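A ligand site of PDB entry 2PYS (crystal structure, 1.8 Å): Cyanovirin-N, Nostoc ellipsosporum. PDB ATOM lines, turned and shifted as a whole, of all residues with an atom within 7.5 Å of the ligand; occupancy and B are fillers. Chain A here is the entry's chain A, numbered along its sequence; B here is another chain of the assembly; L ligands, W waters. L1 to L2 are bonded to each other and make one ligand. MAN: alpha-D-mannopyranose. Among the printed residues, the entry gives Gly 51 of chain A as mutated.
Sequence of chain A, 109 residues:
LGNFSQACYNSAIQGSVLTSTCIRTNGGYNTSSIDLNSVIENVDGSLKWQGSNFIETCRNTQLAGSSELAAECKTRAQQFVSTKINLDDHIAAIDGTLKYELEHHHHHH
The backbone NH of Asn 42 is in hydrogen-bond range of an oxygen (O3) of MAN L2 (3.1 Å).
The backbone carbonyl oxygen of Asn 42 lies within hydrogen-bond range of an oxygen (O3) of MAN L1, 2.6 Å away.
O of Asn 53 sits at hydrogen-bond distance from O4 of MAN L2 (2.7 Å).
O of Lys 74 is in hydrogen-bond range of O4 of MAN L1 (2.7 Å).
An oxygen (O4) of MAN L2 sits at hydrogen-bond distance from the side-chain hydroxyl of Thr 57 (2.7 Å).
The backbone carbonyl oxygen (O) of Ser 52 is in hydrogen-bond range of an oxygen (O3) of MAN L2 (2.8 Å).
An oxygen (O3) of MAN L1 is in hydrogen-bond range of the backbone NH (N) of Asp 44, at 2.9 Å.
An oxygen (O6) of MAN L1 lies within hydrogen-bond range of the side-chain amide oxygen (OE1) of Gln 78.
An oxygen (O3) of MAN L2 lies within hydrogen-bond range of the backbone NH (N) of Phe 54 (3.2 Å).
An oxygen (O4) of MAN L1 lies within hydrogen-bond range of the backbone NH (N) of Arg 76, 3.4 Å away.
The side-chain hydroxyl (OG1) of Thr 57 lies within hydrogen-bond range of the side-chain amide nitrogen (ND2) of Asn 42 (2.8 Å).
The backbone NH of Gly 45 is in hydrogen-bond range of the side-chain amide oxygen of Asn 42 (2.7 Å).
N of Asn 53 sits at hydrogen-bond distance from O of Asn 37 (3.0 Å).
The backbone carbonyl oxygen (O) of Thr 57 is in hydrogen-bond range of the backbone NH (N) of Lys 74, 2.9 Å away.
N of Gly 45 lies within hydrogen-bond range of O of Lys 74, at 3.4 Å.
The side-chain hydroxyl (OG1) of Thr 75 lies within hydrogen-bond range of the backbone NH (N) of Gln 78 (3.5 Å).
The side-chain hydroxyl (OG1) of Thr 75 sits close to the backbone NH (N) of Ala 77, at 3.4 Å.
The side-chain hydroxyl of Thr 75 lies within hydrogen-bond range of the backbone NH of Gln 79, at 3.3 Å.
CG of Glu 41 touches O3 of MAN L2, 3.5 Å away.
CA of Val 43 touches O3 of MAN L1, 3.3 Å away.
N of Gly 45 touches O4 of MAN L1, at 3.9 Å.
OE1 of Glu 56 of chain A touches C6 of MAN L2, at 3.3 Å.
C of Thr 75 touches O4 of MAN L1, 3.3 Å away.
The nearest printed residue that does not touch the ligand is Ile 40 (4.8 Å).
Water W2 bridges an oxygen (O2) of MAN L2 (2.6 Å) and the side-chain amide nitrogen (ND2) of Asn 53 (3.1 Å).
Water W5 lies within hydrogen-bond range of an oxygen (O3) of MAN L1 (2.7 Å) and the guanidinium group of Arg 76 (3.0 Å).
Water W1 lies within hydrogen-bond range of the side-chain carboxylate of Glu 56 of chain A and an oxygen (O6) of MAN L2.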
ATOM      1  N   ASN A  37     -22.043 -29.486 -17.885  1.00  0.00           N
ATOM      2  CA  ASN A  37     -21.707 -30.216 -19.076  1.00  0.00           C
ATOM      3  C   ASN A  37     -22.826 -31.139 -19.555  1.00  0.00           C
ATOM      4  O   ASN A  37     -22.796 -31.598 -20.691  1.00  0.00           O
ATOM      5  CB  ASN A  37     -20.451 -31.065 -18.800  1.00  0.00           C
ATOM      6  CG  ASN A  37     -19.808 -31.610 -20.054  1.00  0.00           C
ATOM      7  OD1 ASN A  37     -19.670 -30.899 -21.075  1.00  0.00           O
ATOM      8  ND2 ASN A  37     -19.302 -32.813 -19.955  1.00  0.00           N
ATOM      9  N   ILE A  40     -25.115 -28.068 -21.690  1.00  0.00           N
ATOM     10  CA  ILE A  40     -24.524 -27.084 -22.606  1.00  0.00           C
ATOM     11  C   ILE A  40     -23.649 -27.744 -23.620  1.00  0.00           C
ATOM     12  O   ILE A  40     -22.795 -28.595 -23.288  1.00  0.00           O
ATOM     13  CB  ILE A  40     -23.737 -26.040 -21.839  1.00  0.00           C
ATOM     14  CG1 ILE A  40     -24.688 -25.269 -20.902  1.00  0.00           C
ATOM     15  CG2 ILE A  40     -22.972 -25.124 -22.844  1.00  0.00           C
ATOM     16  CD1 ILE A  40     -24.014 -24.308 -19.912  1.00  0.00           C
ATOM     17  N   GLU A  41     -23.824 -27.322 -24.870  1.00  0.00           N
ATOM     18  CA  GLU A  41     -23.093 -27.918 -26.002  1.00  0.00           C
ATOM     19  C   GLU A  41     -22.204 -26.840 -26.617  1.00  0.00           C
ATOM     20  O   GLU A  41     -22.615 -25.684 -26.695  1.00  0.00           O
ATOM     21  CB  GLU A  41     -24.062 -28.435 -27.095  1.00  0.00           C
ATOM     22  CG  GLU A  41     -23.363 -29.235 -28.203  1.00  0.00           C
ATOM     23  CD  GLU A  41     -24.259 -29.669 -29.382  1.00  0.00           C
ATOM     24  OE1 GLU A  41     -25.487 -29.720 -29.192  1.00  0.00           O
ATOM     25  OE2 GLU A  41     -23.718 -30.001 -30.485  1.00  0.00           O
ATOM     26  N   ASN A  42     -21.003 -27.232 -27.040  1.00  0.00           N
ATOM     27  CA  ASN A  42     -20.176 -26.373 -27.914  1.00  0.00           C
ATOM     28  C   ASN A  42     -20.609 -26.614 -29.369  1.00  0.00           C
ATOM     29  O   ASN A  42     -20.289 -27.632 -29.934  1.00  0.00           O
ATOM     30  CB  ASN A  42     -18.679 -26.657 -27.729  1.00  0.00           C
ATOM     31  CG  ASN A  42     -17.815 -26.039 -28.818  1.00  0.00           C
ATOM     32  OD1 ASN A  42     -18.282 -25.129 -29.517  1.00  0.00           O
ATOM     33  ND2 ASN A  42     -16.560 -26.520 -28.968  1.00  0.00           N
ATOM     34  N   VAL A  43     -21.373 -25.680 -29.945  1.00  0.00           N
ATOM     35  CA  VAL A  43     -21.744 -25.757 -31.332  1.00  0.00           C
ATOM     36  C   VAL A  43     -20.881 -24.762 -32.120  1.00  0.00           C
ATOM     37  O   VAL A  43     -21.143 -23.570 -32.113  1.00  0.00           O
ATOM     38  CB  VAL A  43     -23.250 -25.487 -31.569  1.00  0.00           C
ATOM     39  CG1 VAL A  43     -23.617 -25.652 -33.033  1.00  0.00           C
ATOM     40  CG2 VAL A  43     -24.112 -26.359 -30.693  1.00  0.00           C
ATOM     41  N   ASP A  44     -19.878 -25.298 -32.813  1.00  0.00           N
ATOM     42  CA  ASP A  44     -18.973 -24.550 -33.688  1.00  0.00           C
ATOM     43  C   ASP A  44     -18.307 -23.366 -32.997  1.00  0.00           C
ATOM     44  O   ASP A  44     -18.062 -22.362 -33.640  1.00  0.00           O
ATOM     45  CB  ASP A  44     -19.721 -24.088 -34.939  1.00  0.00           C
ATOM     46  CG  ASP A  44     -18.802 -23.712 -36.098  1.00  0.00           C
ATOM     47  OD1 ASP A  44     -17.677 -24.219 -36.198  1.00  0.00           O
ATOM     48  OD2 ASP A  44     -19.258 -22.902 -36.921  1.00  0.00           O
ATOM     49  N   GLY A  45     -17.972 -23.537 -31.719  1.00  0.00           N
ATOM     50  CA  GLY A  45     -17.300 -22.509 -30.917  1.00  0.00           C
ATOM     51  C   GLY A  45     -18.205 -21.732 -29.977  1.00  0.00           C
ATOM     52  O   GLY A  45     -17.701 -21.002 -29.094  1.00  0.00           O
ATOM     53  N   SER A  46     -19.528 -21.815 -30.152  1.00  0.00           N
ATOM     54  CA  SER A  46     -20.481 -21.102 -29.351  1.00  0.00           C
ATOM     55  C   SER A  46     -21.192 -22.024 -28.390  1.00  0.00           C
ATOM     56  O   SER A  46     -21.696 -23.074 -28.786  1.00  0.00           O
ATOM     57  CB  SER A  46     -21.540 -20.455 -30.207  1.00  0.00           C
ATOM     58  OG  SER A  46     -20.950 -19.442 -31.033  1.00  0.00           O
ATOM     59  N   LEU A  47     -21.260 -21.606 -27.135  1.00  0.00           N
ATOM     60  CA  LEU A  47     -22.057 -22.304 -26.115  1.00  0.00           C
ATOM     61  C   LEU A  47     -23.563 -22.146 -26.374  1.00  0.00           C
ATOM     62  O   LEU A  47     -24.069 -21.034 -26.581  1.00  0.00           O
ATOM     63  CB  LEU A  47     -21.711 -21.788 -24.735  1.00  0.00           C
ATOM     64  CG  LEU A  47     -20.260 -22.039 -24.311  1.00  0.00           C
ATOM     65  CD1 LEU A  47     -19.909 -21.220 -23.054  1.00  0.00           C
ATOM     66  CD2 LEU A  47     -19.913 -23.517 -24.091  1.00  0.00           C
ATOM     67  N   GLY A  51     -28.060 -29.474 -25.513  1.00  0.00           N
ATOM     68  CA  GLY A  51     -27.066 -30.474 -25.819  1.00  0.00           C
ATOM     69  C   GLY A  51     -26.108 -30.619 -24.673  1.00  0.00           C
ATOM     70  O   GLY A  51     -26.367 -30.130 -23.615  1.00  0.00           O
ATOM     71  N   SER A  52     -24.981 -31.291 -24.879  1.00  0.00           N
ATOM     72  CA  SER A  52     -24.026 -31.599 -23.847  1.00  0.00           C
ATOM     73  C   SER A  52     -22.564 -31.585 -24.354  1.00  0.00           C
ATOM     74  O   SER A  52     -22.313 -31.440 -25.569  1.00  0.00           O
ATOM     75  CB  SER A  52     -24.341 -33.013 -23.328  1.00  0.00           C
ATOM     76  OG  SER A  52     -25.711 -33.136 -23.043  1.00  0.00           O
ATOM     77  N   ASN A  53     -21.636 -31.767 -23.406  1.00  0.00           N
ATOM     78  CA  ASN A  53     -20.274 -32.234 -23.631  1.00  0.00           C
ATOM     79  C   ASN A  53     -19.321 -31.113 -24.094  1.00  0.00           C
ATOM     80  O   ASN A  53     -18.223 -31.391 -24.603  1.00  0.00           O
ATOM     81  CB  ASN A  53     -20.234 -33.393 -24.639  1.00  0.00           C
ATOM     82  CG  ASN A  53     -20.962 -34.642 -24.119  1.00  0.00           C
ATOM     83  OD1 ASN A  53     -20.742 -35.039 -22.981  1.00  0.00           O
ATOM     84  ND2 ASN A  53     -21.823 -35.246 -24.940  1.00  0.00           N
ATOM     85  N   PHE A  54     -19.746 -29.881 -23.908  1.00  0.00           N
ATOM     86  CA  PHE A  54     -18.887 -28.714 -24.252  1.00  0.00           C
ATOM     87  C   PHE A  54     -17.496 -28.764 -23.652  1.00  0.00           C
ATOM     88  O   PHE A  54     -16.551 -28.213 -24.227  1.00  0.00           O
ATOM     89  CB  PHE A  54     -19.605 -27.417 -23.886  1.00  0.00           C
ATOM     90  CG  PHE A  54     -19.453 -26.991 -22.437  1.00  0.00           C
ATOM     91  CD1 PHE A  54     -18.444 -26.123 -22.071  1.00  0.00           C
ATOM     92  CD2 PHE A  54     -20.315 -27.459 -21.463  1.00  0.00           C
ATOM     93  CE1 PHE A  54     -18.318 -25.721 -20.723  1.00  0.00           C
ATOM     94  CE2 PHE A  54     -20.205 -27.053 -20.152  1.00  0.00           C
ATOM     95  CZ  PHE A  54     -19.190 -26.177 -19.788  1.00  0.00           C
ATOM     96  N   ILE A  55     -17.350 -29.333 -22.459  1.00  0.00           N
ATOM     97  CA  ILE A  55     -16.039 -29.324 -21.756  1.00  0.00           C
ATOM     98  C   ILE A  55     -14.902 -30.072 -22.537  1.00  0.00           C
ATOM     99  O   ILE A  55     -13.704 -29.764 -22.385  1.00  0.00           O
ATOM    100  CB  ILE A  55     -16.229 -29.856 -20.292  1.00  0.00           C
ATOM    101  CG1 ILE A  55     -15.232 -29.231 -19.307  1.00  0.00           C
ATOM    102  CG2 ILE A  55     -16.173 -31.425 -20.256  1.00  0.00           C
ATOM    103  CD1 ILE A  55     -15.314 -27.722 -19.221  1.00  0.00           C
ATOM    104  N   GLU A  56     -15.291 -31.040 -23.372  1.00  0.00           N
ATOM    105  CA  GLU A  56     -14.358 -31.803 -24.192  1.00  0.00           C
ATOM    106  C   GLU A  56     -13.613 -30.938 -25.217  1.00  0.00           C
ATOM    107  O   GLU A  56     -12.515 -31.308 -25.693  1.00  0.00           O
ATOM    108  CB  GLU A  56     -15.076 -32.904 -24.951  1.00  0.00           C
ATOM    109  CG  GLU A  56     -15.725 -33.964 -24.063  1.00  0.00           C
ATOM    110  CD  GLU A  56     -16.417 -35.059 -24.832  1.00  0.00           C
ATOM    111  OE1 GLU A  56     -16.353 -35.087 -26.087  1.00  0.00           O
ATOM    112  OE2 GLU A  56     -17.044 -35.917 -24.180  1.00  0.00           O
ATOM    113  N   THR A  57     -14.227 -29.829 -25.586  1.00  0.00           N
ATOM    114  CA  THR A  57     -13.693 -29.001 -26.658  1.00  0.00           C
ATOM    115  C   THR A  57     -13.620 -27.515 -26.301  1.00  0.00           C
ATOM    116  O   THR A  57     -13.495 -26.626 -27.179  1.00  0.00           O
ATOM    117  CB  THR A  57     -14.456 -29.245 -27.990  1.00  0.00           C
ATOM    118  OG1 THR A  57     -15.836 -28.981 -27.823  1.00  0.00           O
ATOM    119  CG2 THR A  57     -14.211 -30.683 -28.537  1.00  0.00           C
ATOM    120  N   CYS A  58     -13.682 -27.239 -25.009  1.00  0.00           N
ATOM    121  CA  CYS A  58     -13.557 -25.868 -24.479  1.00  0.00           C
ATOM    122  C   CYS A  58     -12.503 -25.782 -23.380  1.00  0.00           C
ATOM    123  O   CYS A  58     -12.109 -26.807 -22.793  1.00  0.00           O
ATOM    124  CB  CYS A  58     -14.906 -25.332 -24.002  1.00  0.00           C
ATOM    125  SG  CYS A  58     -16.290 -25.275 -25.201  1.00  0.00           S
ATOM    126  N   CYS A  73     -13.726 -21.962 -26.910  1.00  0.00           N
ATOM    127  CA  CYS A  73     -14.184 -23.215 -27.476  1.00  0.00           C
ATOM    128  C   CYS A  73     -13.717 -23.358 -28.908  1.00  0.00           C
ATOM    129  O   CYS A  73     -13.480 -22.336 -29.622  1.00  0.00           O
ATOM    130  CB  CYS A  73     -15.698 -23.312 -27.391  1.00  0.00           C
ATOM    131  SG  CYS A  73     -16.438 -23.320 -25.767  1.00  0.00           S
ATOM    132  N   LYS A  74     -13.550 -24.613 -29.317  1.00  0.00           N
ATOM    133  CA  LYS A  74     -13.097 -24.935 -30.642  1.00  0.00           C
ATOM    134  C   LYS A  74     -14.247 -24.968 -31.664  1.00  0.00           C
ATOM    135  O   LYS A  74     -15.276 -25.612 -31.477  1.00  0.00           O
ATOM    136  CB  LYS A  74     -12.407 -26.326 -30.649  1.00  0.00           C
ATOM    137  CG  LYS A  74     -10.990 -26.361 -30.156  1.00  0.00           C
ATOM    138  CD  LYS A  74     -10.222 -27.636 -30.616  1.00  0.00           C
ATOM    139  CE  LYS A  74     -11.010 -28.939 -30.305  1.00  0.00           C
ATOM    140  NZ  LYS A  74     -10.198 -30.183 -30.476  1.00  0.00           N
ATOM    141  N   THR A  75     -14.026 -24.320 -32.802  1.00  0.00           N
ATOM    142  CA  THR A  75     -14.927 -24.388 -33.918  1.00  0.00           C
ATOM    143  C   THR A  75     -14.756 -25.759 -34.580  1.00  0.00           C
ATOM    144  O   THR A  75     -13.848 -26.520 -34.217  1.00  0.00           O
ATOM    145  CB  THR A  75     -14.594 -23.280 -34.977  1.00  0.00           C
ATOM    146  OG1 THR A  75     -13.283 -23.548 -35.528  1.00  0.00           O
ATOM    147  CG2 THR A  75     -14.641 -21.883 -34.319  1.00  0.00           C
ATOM    148  N   ARG A  76     -15.588 -26.071 -35.566  1.00  0.00           N
ATOM    149  CA  ARG A  76     -15.457 -27.342 -36.298  1.00  0.00           C
ATOM    150  C   ARG A  76     -14.134 -27.455 -37.033  1.00  0.00           C
ATOM    151  O   ARG A  76     -13.563 -28.514 -37.130  1.00  0.00           O
ATOM    152  CB  ARG A  76     -16.650 -27.553 -37.245  1.00  0.00           C
ATOM    153  CG  ARG A  76     -17.869 -28.037 -36.486  1.00  0.00           C
ATOM    154  CD  ARG A  76     -19.042 -28.372 -37.368  1.00  0.00           C
ATOM    155  NE  ARG A  76     -19.582 -27.216 -38.044  1.00  0.00           N
ATOM    156  CZ  ARG A  76     -20.698 -26.556 -37.714  1.00  0.00           C
ATOM    157  NH1 ARG A  76     -21.461 -26.915 -36.704  1.00  0.00           N
ATOM    158  NH2 ARG A  76     -21.062 -25.525 -38.443  1.00  0.00           N
ATOM    159  N   ALA A  77     -13.619 -26.310 -37.500  1.00  0.00           N
ATOM    160  CA  ALA A  77     -12.292 -26.221 -38.096  1.00  0.00           C
ATOM    161  C   ALA A  77     -11.144 -26.151 -37.080  1.00  0.00           C
ATOM    162  O   ALA A  77     -10.004 -25.852 -37.447  1.00  0.00           O
ATOM    163  CB  ALA A  77     -12.258 -25.037 -39.089  1.00  0.00           C
ATOM    164  N   GLN A  78     -11.428 -26.447 -35.813  1.00  0.00           N
ATOM    165  CA  GLN A  78     -10.403 -26.630 -34.775  1.00  0.00           C
ATOM    166  C   GLN A  78      -9.633 -25.352 -34.344  1.00  0.00           C
ATOM    167  O   GLN A  78      -8.494 -25.412 -33.946  1.00  0.00           O
ATOM    168  CB  GLN A  78      -9.440 -27.737 -35.199  1.00  0.00           C
ATOM    169  CG  GLN A  78     -10.162 -29.016 -35.585  1.00  0.00           C
ATOM    170  CD  GLN A  78     -11.014 -29.548 -34.437  1.00  0.00           C
ATOM    171  OE1 GLN A  78     -12.234 -29.565 -34.528  1.00  0.00           O
ATOM    172  NE2 GLN A  78     -10.381 -29.952 -33.372  1.00  0.00           N
ATOM    173  N   GLN A  79     -10.277 -24.190 -34.445  1.00  0.00           N
ATOM    174  CA  GLN A  79      -9.682 -22.980 -33.885  1.00  0.00           C
ATOM    175  C   GLN A  79     -10.520 -22.454 -32.728  1.00  0.00           C
ATOM    176  O   GLN A  79     -11.694 -22.723 -32.615  1.00  0.00           O
ATOM    177  CB  GLN A  79      -9.488 -21.894 -34.976  1.00  0.00           C
ATOM    178  CG  GLN A  79      -8.584 -22.301 -36.180  1.00  0.00           C
ATOM    179  CD  GLN A  79      -8.332 -21.148 -37.146  1.00  0.00           C
ATOM    180  OE1 GLN A  79      -8.762 -20.013 -36.903  1.00  0.00           O
ATOM    181  NE2 GLN A  79      -7.666 -21.445 -38.263  1.00  0.00           N
ATOM    182  N   GLU B  56      -8.865 -36.023 -22.021  1.00  0.00           N
ATOM    183  CA  GLU B  56      -8.352 -35.836 -23.393  1.00  0.00           C
ATOM    184  C   GLU B  56      -6.866 -36.214 -23.528  1.00  0.00           C
ATOM    185  O   GLU B  56      -6.426 -36.608 -24.607  1.00  0.00           O
ATOM    186  CB  GLU B  56      -8.536 -34.376 -23.801  1.00  0.00           C
ATOM    187  CG  GLU B  56      -8.082 -33.993 -25.182  1.00  0.00           C
ATOM    188  CD  GLU B  56      -8.971 -34.553 -26.291  1.00  0.00           C
ATOM    189  OE1 GLU B  56     -10.103 -34.997 -25.964  1.00  0.00           O
ATOM    190  OE2 GLU B  56      -8.542 -34.534 -27.472  1.00  0.00           O
HETATM  191  C1  MAN L   1     -17.573 -31.107 -32.791  1.00  0.00           C
HETATM  192  C2  MAN L   1     -18.886 -30.491 -32.418  1.00  0.00           C
HETATM  193  C3  MAN L   1     -18.659 -29.010 -32.807  1.00  0.00           C
HETATM  194  C4  MAN L   1     -17.352 -28.498 -32.221  1.00  0.00           C
HETATM  195  C5  MAN L   1     -16.161 -29.453 -32.494  1.00  0.00           C
HETATM  196  C6  MAN L   1     -14.897 -28.910 -31.822  1.00  0.00           C
HETATM  197  O1  MAN L   1     -17.393 -31.622 -34.026  1.00  0.00           O
HETATM  198  O2  MAN L   1     -19.030 -30.529 -31.007  1.00  0.00           O
HETATM  199  O3  MAN L   1     -19.772 -28.203 -32.452  1.00  0.00           O
HETATM  200  O4  MAN L   1     -17.071 -27.166 -32.714  1.00  0.00           O
HETATM  201  O5  MAN L   1     -16.418 -30.803 -32.090  1.00  0.00           O
HETATM  202  O6  MAN L   1     -13.857 -29.794 -32.048  1.00  0.00           O
HETATM  203  C1  MAN L   2     -19.748 -31.663 -30.479  1.00  0.00           C
HETATM  204  C2  MAN L   2     -20.525 -31.210 -29.224  1.00  0.00           C
HETATM  205  C3  MAN L   2     -19.554 -30.613 -28.220  1.00  0.00           C
HETATM  206  C4  MAN L   2     -18.452 -31.620 -27.909  1.00  0.00           C
HETATM  207  C5  MAN L   2     -17.836 -32.214 -29.200  1.00  0.00           C
HETATM  208  C6  MAN L   2     -16.886 -33.377 -28.909  1.00  0.00           C
HETATM  209  O2  MAN L   2     -21.223 -32.275 -28.566  1.00  0.00           O
HETATM  210  O3  MAN L   2     -20.251 -30.214 -27.047  1.00  0.00           O
HETATM  211  O4  MAN L   2     -17.437 -31.016 -27.129  1.00  0.00           O
HETATM  212  O5  MAN L   2     -18.811 -32.664 -30.132  1.00  0.00           O
HETATM  213  O6  MAN L   2     -16.107 -33.622 -30.066  1.00  0.00           O
HETATM  214  O   HOH W   1     -14.098 -35.025 -27.975  1.00  0.00           O
HETATM  215  O   HOH W   2     -20.761 -34.677 -27.829  1.00  0.00           O
HETATM  216  O   HOH W   3     -14.076 -32.626 -31.448  1.00  0.00           O
HETATM  217  O   HOH W   4     -18.484 -34.784 -32.381  1.00  0.00           O
HETATM  218  O   HOH W   5     -21.561 -28.808 -34.382  1.00  0.00           O
